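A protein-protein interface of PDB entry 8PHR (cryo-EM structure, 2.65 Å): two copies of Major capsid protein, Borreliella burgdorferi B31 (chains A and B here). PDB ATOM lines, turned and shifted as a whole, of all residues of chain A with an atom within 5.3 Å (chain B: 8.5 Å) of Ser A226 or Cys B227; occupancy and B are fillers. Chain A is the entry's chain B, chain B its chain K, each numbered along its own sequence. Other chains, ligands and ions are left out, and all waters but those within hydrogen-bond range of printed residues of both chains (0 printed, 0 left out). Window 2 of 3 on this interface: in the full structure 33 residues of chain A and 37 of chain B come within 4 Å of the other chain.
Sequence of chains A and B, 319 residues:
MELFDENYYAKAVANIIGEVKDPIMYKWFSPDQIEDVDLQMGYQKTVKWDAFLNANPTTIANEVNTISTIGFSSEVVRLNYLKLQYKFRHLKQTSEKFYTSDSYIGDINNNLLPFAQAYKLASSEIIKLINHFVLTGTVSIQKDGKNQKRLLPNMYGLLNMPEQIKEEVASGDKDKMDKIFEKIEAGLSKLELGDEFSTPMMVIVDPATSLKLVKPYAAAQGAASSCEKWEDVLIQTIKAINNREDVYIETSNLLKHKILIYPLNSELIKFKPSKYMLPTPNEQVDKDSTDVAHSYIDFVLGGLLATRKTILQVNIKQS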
ATOM      1  N   TYR A 217       3.310 -23.989  23.513  1.00  0.00           N
ATOM      2  CA  TYR A 217       1.894 -23.837  23.211  1.00  0.00           C
ATOM      3  C   TYR A 217       1.620 -24.236  21.766  1.00  0.00           C
ATOM      4  O   TYR A 217       2.318 -23.799  20.846  1.00  0.00           O
ATOM      5  CB  TYR A 217       1.450 -22.395  23.460  1.00  0.00           C
ATOM      6  CG  TYR A 217       0.105 -22.047  22.860  1.00  0.00           C
ATOM      7  CD1 TYR A 217      -1.024 -22.803  23.155  1.00  0.00           C
ATOM      8  CD2 TYR A 217      -0.038 -20.966  22.002  1.00  0.00           C
ATOM      9  CE1 TYR A 217      -2.256 -22.491  22.611  1.00  0.00           C
ATOM     10  CE2 TYR A 217      -1.266 -20.646  21.453  1.00  0.00           C
ATOM     11  CZ  TYR A 217      -2.371 -21.412  21.761  1.00  0.00           C
ATOM     12  OH  TYR A 217      -3.595 -21.097  21.217  1.00  0.00           O
ATOM     13  N   ALA A 224       1.920 -26.428  15.425  1.00  0.00           N
ATOM     14  CA  ALA A 224       2.605 -25.998  16.634  1.00  0.00           C
ATOM     15  C   ALA A 224       3.163 -24.596  16.428  1.00  0.00           C
ATOM     16  O   ALA A 224       3.252 -24.094  15.304  1.00  0.00           O
ATOM     17  CB  ALA A 224       3.725 -26.970  17.022  1.00  0.00           C
ATOM     18  N   SER A 225       3.546 -23.966  17.535  1.00  0.00           N
ATOM     19  CA  SER A 225       4.094 -22.616  17.515  1.00  0.00           C
ATOM     20  C   SER A 225       5.322 -22.587  18.419  1.00  0.00           C
ATOM     21  O   SER A 225       5.801 -23.626  18.882  1.00  0.00           O
ATOM     22  CB  SER A 225       3.031 -21.592  17.941  1.00  0.00           C
ATOM     23  OG  SER A 225       2.741 -21.704  19.323  1.00  0.00           O
ATOM     24  N   SER A 226       5.835 -21.385  18.670  1.00  0.00           N
ATOM     25  CA  SER A 226       7.016 -21.215  19.503  1.00  0.00           C
ATOM     26  C   SER A 226       6.935 -19.870  20.209  1.00  0.00           C
ATOM     27  O   SER A 226       6.017 -19.077  19.982  1.00  0.00           O
ATOM     28  CB  SER A 226       8.303 -21.323  18.678  1.00  0.00           C
ATOM     29  OG  SER A 226       8.397 -20.266  17.739  1.00  0.00           O
ATOM     30  N   CYS A 227       7.910 -19.630  21.087  1.00  0.00           N
ATOM     31  CA  CYS A 227       8.037 -18.393  21.857  1.00  0.00           C
ATOM     32  C   CYS A 227       6.848 -18.156  22.783  1.00  0.00           C
ATOM     33  O   CYS A 227       6.618 -17.026  23.227  1.00  0.00           O
ATOM     34  CB  CYS A 227       8.242 -17.182  20.938  1.00  0.00           C
ATOM     35  SG  CYS A 227       9.652 -17.328  19.816  1.00  0.00           S
ATOM     36  N   GLU A 228       6.085 -19.205  23.087  1.00  0.00           N
ATOM     37  CA  GLU A 228       4.953 -19.099  23.995  1.00  0.00           C
ATOM     38  C   GLU A 228       4.627 -20.488  24.522  1.00  0.00           C
ATOM     39  O   GLU A 228       4.680 -21.467  23.772  1.00  0.00           O
ATOM     40  CB  GLU A 228       3.731 -18.485  23.302  1.00  0.00           C
ATOM     41  CG  GLU A 228       2.576 -18.176  24.242  1.00  0.00           C
ATOM     42  CD  GLU A 228       1.317 -17.774  23.501  1.00  0.00           C
ATOM     43  OE1 GLU A 228       1.331 -17.783  22.253  1.00  0.00           O
ATOM     44  OE2 GLU A 228       0.311 -17.450  24.169  1.00  0.00           O
ATOM     45  N   PRO B 216      -7.024 -16.583  20.584  1.00  0.00           N
ATOM     46  CA  PRO B 216      -6.098 -16.251  19.494  1.00  0.00           C
ATOM     47  C   PRO B 216      -6.815 -15.593  18.324  1.00  0.00           C
ATOM     48  O   PRO B 216      -7.961 -15.920  18.007  1.00  0.00           O
ATOM     49  CB  PRO B 216      -5.508 -17.612  19.101  1.00  0.00           C
ATOM     50  CG  PRO B 216      -5.741 -18.490  20.293  1.00  0.00           C
ATOM     51  CD  PRO B 216      -7.038 -18.025  20.875  1.00  0.00           C
ATOM     52  N   TYR B 217      -6.123 -14.653  17.685  1.00  0.00           N
ATOM     53  CA  TYR B 217      -6.692 -13.935  16.553  1.00  0.00           C
ATOM     54  C   TYR B 217      -6.882 -14.878  15.371  1.00  0.00           C
ATOM     55  O   TYR B 217      -6.001 -15.685  15.058  1.00  0.00           O
ATOM     56  CB  TYR B 217      -5.788 -12.765  16.162  1.00  0.00           C
ATOM     57  CG  TYR B 217      -6.112 -12.154  14.816  1.00  0.00           C
ATOM     58  CD1 TYR B 217      -7.374 -11.636  14.553  1.00  0.00           C
ATOM     59  CD2 TYR B 217      -5.157 -12.095  13.811  1.00  0.00           C
ATOM     60  CE1 TYR B 217      -7.673 -11.075  13.325  1.00  0.00           C
ATOM     61  CE2 TYR B 217      -5.447 -11.536  12.580  1.00  0.00           C
ATOM     62  CZ  TYR B 217      -6.708 -11.028  12.343  1.00  0.00           C
ATOM     63  OH  TYR B 217      -7.002 -10.471  11.119  1.00  0.00           O
ATOM     64  N   ALA B 224      -6.074 -20.164  13.584  1.00  0.00           N
ATOM     65  CA  ALA B 224      -5.580 -19.445  14.750  1.00  0.00           C
ATOM     66  C   ALA B 224      -4.160 -18.948  14.511  1.00  0.00           C
ATOM     67  O   ALA B 224      -3.316 -19.661  13.961  1.00  0.00           O
ATOM     68  CB  ALA B 224      -5.624 -20.344  15.985  1.00  0.00           C
ATOM     69  N   SER B 225      -3.900 -17.713  14.929  1.00  0.00           N
ATOM     70  CA  SER B 225      -2.589 -17.109  14.754  1.00  0.00           C
ATOM     71  C   SER B 225      -1.643 -17.565  15.863  1.00  0.00           C
ATOM     72  O   SER B 225      -2.034 -18.251  16.813  1.00  0.00           O
ATOM     73  CB  SER B 225      -2.707 -15.587  14.723  1.00  0.00           C
ATOM     74  OG  SER B 225      -3.570 -15.164  13.683  1.00  0.00           O
ATOM     75  N   SER B 226      -0.378 -17.173  15.743  1.00  0.00           N
ATOM     76  CA  SER B 226       0.645 -17.480  16.732  1.00  0.00           C
ATOM     77  C   SER B 226       1.139 -16.182  17.352  1.00  0.00           C
ATOM     78  O   SER B 226       1.550 -15.264  16.632  1.00  0.00           O
ATOM     79  CB  SER B 226       1.811 -18.249  16.102  1.00  0.00           C
ATOM     80  OG  SER B 226       1.355 -19.425  15.455  1.00  0.00           O
ATOM     81  N   CYS B 227       1.088 -16.108  18.683  1.00  0.00           N
ATOM     82  CA  CYS B 227       1.504 -14.935  19.451  1.00  0.00           C
ATOM     83  C   CYS B 227       0.720 -13.680  19.076  1.00  0.00           C
ATOM     84  O   CYS B 227       1.157 -12.562  19.364  1.00  0.00           O
ATOM     85  CB  CYS B 227       3.011 -14.679  19.306  1.00  0.00           C
ATOM     86  SG  CYS B 227       4.057 -16.039  19.876  1.00  0.00           S
ATOM     87  N   GLU B 228      -0.435 -13.843  18.434  1.00  0.00           N
ATOM     88  CA  GLU B 228      -1.288 -12.727  18.040  1.00  0.00           C
ATOM     89  C   GLU B 228      -2.699 -12.995  18.538  1.00  0.00           C
ATOM     90  O   GLU B 228      -3.326 -13.978  18.128  1.00  0.00           O
ATOM     91  CB  GLU B 228      -1.278 -12.528  16.522  1.00  0.00           C
ATOM     92  CG  GLU B 228      -0.033 -11.833  15.999  1.00  0.00           C
ATOM     93  CD  GLU B 228       0.269 -10.545  16.740  1.00  0.00           C
ATOM     94  OE1 GLU B 228      -0.623  -9.670  16.803  1.00  0.00           O
ATOM     95  OE2 GLU B 228       1.395 -10.405  17.260  1.00  0.00           O
ATOM     96  N   LYS B 229      -3.194 -12.128  19.415  1.00  0.00           N
ATOM     97  CA  LYS B 229      -4.511 -12.280  20.008  1.00  0.00           C
ATOM     98  C   LYS B 229      -5.378 -11.069  19.688  1.00  0.00           C
ATOM     99  O   LYS B 229      -4.890 -10.024  19.245  1.00  0.00           O
ATOM    100  CB  LYS B 229      -4.416 -12.478  21.526  1.00  0.00           C
ATOM    101  CG  LYS B 229      -3.545 -13.654  21.936  1.00  0.00           C
ATOM    102  CD  LYS B 229      -3.050 -13.508  23.363  1.00  0.00           C
ATOM    103  CE  LYS B 229      -2.054 -14.602  23.711  1.00  0.00           C
ATOM    104  NZ  LYS B 229      -1.530 -14.459  25.097  1.00  0.00           N
ATOM    105  N   TRP B 230      -6.685 -11.235  19.915  1.00  0.00           N
ATOM    106  CA  TRP B 230      -7.635 -10.165  19.632  1.00  0.00           C
ATOM    107  C   TRP B 230      -7.323  -8.917  20.449  1.00  0.00           C
ATOM    108  O   TRP B 230      -7.491  -7.793  19.965  1.00  0.00           O
ATOM    109  CB  TRP B 230      -9.059 -10.643  19.908  1.00  0.00           C
ATOM    110  CG  TRP B 230      -9.595 -11.567  18.859  1.00  0.00           C
ATOM    111  CD1 TRP B 230      -9.827 -12.905  18.988  1.00  0.00           C
ATOM    112  CD2 TRP B 230      -9.965 -11.223  17.520  1.00  0.00           C
ATOM    113  NE1 TRP B 230     -10.319 -13.416  17.811  1.00  0.00           N
ATOM    114  CE2 TRP B 230     -10.414 -12.402  16.894  1.00  0.00           C
ATOM    115  CE3 TRP B 230      -9.963 -10.030  16.788  1.00  0.00           C
ATOM    116  CZ2 TRP B 230     -10.854 -12.426  15.571  1.00  0.00           C
ATOM    117  CZ3 TRP B 230     -10.400 -10.054  15.477  1.00  0.00           C
ATOM    118  CH2 TRP B 230     -10.840 -11.244  14.882  1.00  0.00           C
ATOM    119  N   ASP B 232      -4.320  -7.890  21.432  1.00  0.00           N
ATOM    120  CA  ASP B 232      -3.183  -7.224  20.803  1.00  0.00           C
ATOM    121  C   ASP B 232      -3.598  -6.531  19.512  1.00  0.00           C
ATOM    122  O   ASP B 232      -3.135  -5.421  19.216  1.00  0.00           O
ATOM    123  CB  ASP B 232      -2.064  -8.231  20.537  1.00  0.00           C
ATOM    124  CG  ASP B 232      -1.779  -9.113  21.737  1.00  0.00           C
ATOM    125  OD1 ASP B 232      -1.394  -8.574  22.795  1.00  0.00           O
ATOM    126  OD2 ASP B 232      -1.937 -10.346  21.618  1.00  0.00           O
ATOM    127  N   VAL B 233      -4.469  -7.171  18.728  1.00  0.00           N
ATOM    128  CA  VAL B 233      -4.946  -6.554  17.492  1.00  0.00           C
ATOM    129  C   VAL B 233      -5.715  -5.274  17.799  1.00  0.00           C
ATOM    130  O   VAL B 233      -5.555  -4.257  17.114  1.00  0.00           O
ATOM    131  CB  VAL B 233      -5.797  -7.553  16.687  1.00  0.00           C
ATOM    132  CG1 VAL B 233      -6.360  -6.890  15.442  1.00  0.00           C
ATOM    133  CG2 VAL B 233      -4.970  -8.771  16.309  1.00  0.00           C
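The backbone carbonyl oxygen (O) of Ser A226 sits at hydrogen-bond distance from the side-chain sulfur (SG) of Cys B227, 3.6 Å away. NZ of Lys B229 is in salt-bridge range of OE2 of Glu A228 (3.6 Å).
The backbone carbonyl oxygen (O) of Tyr A217 lies within hydrogen-bond range of the side-chain hydroxyl (OG) of Ser A225, 2.6 Å away. The backbone carbonyl oxygen (O) of Pro B216 is in hydrogen-bond range of the indole nitrogen (NE1) of Trp B230. The backbone NH (N) of Lys B229 lies within hydrogen-bond range of the side-chain carboxylate (OD2) of Asp B232, 3.1 Å away. The backbone carbonyl oxygen (O) of Glu A228 lies within hydrogen-bond range of the backbone NH (N) of Tyr A217 (2.9 Å).
Ser A226 touches just one residue of chain B: Cys B227. Cys B227 touches two residues of chain A. No residue of chain B comes within 4 Å of Cys A227. Of the printed residues of chain A, Ser B226 touches Ser A225. Of the printed residues of chain B, Tyr A217 touches Pro B216 (3.5 Å). Of the printed residues of chain B, Glu A228 touches Cys B227 and Lys B229. Tyr B217 touches none of the printed residues of chain A. Ala B224 touches none of the printed residues of chain A. The nearest residue of chain A that does not touch Cys B227 is Cys A227 (4.3 Å).
Ser A225 touches Ser B226, but with the chains exchanged Ser A226 does not touch Ser B225 (8.7 Å). Ser A226 touches Cys B227, but with the chains exchanged Cys A227 does not touch Ser B226 (8.0 Å). Glu A228 touches Cys B227, but with the chains exchanged Cys A227 does not touch Glu B228 (9.1 Å). 6 positions are printed for both chains.
Hydrophobic or aromatic side chains of chain A that line the printed part of chain B: Tyr A217. Hydrophobic or aromatic side chains of chain B within 4 Å of the printed part of chain A: Pro B216. Among the printed residues, Asp or Glu carboxylates within 4 Å of a Lys or Arg side-chain nitrogen of the other chain: Glu A228 with Lys B229 (3.6 Å).
Among the printed residues, pairs that only touch across the chains: Tyr A217 with Pro B216 (3.5 Å), Ser A225 with Ser B226 (3.7 Å) and Glu A228 with Cys B227 (3.95 Å).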
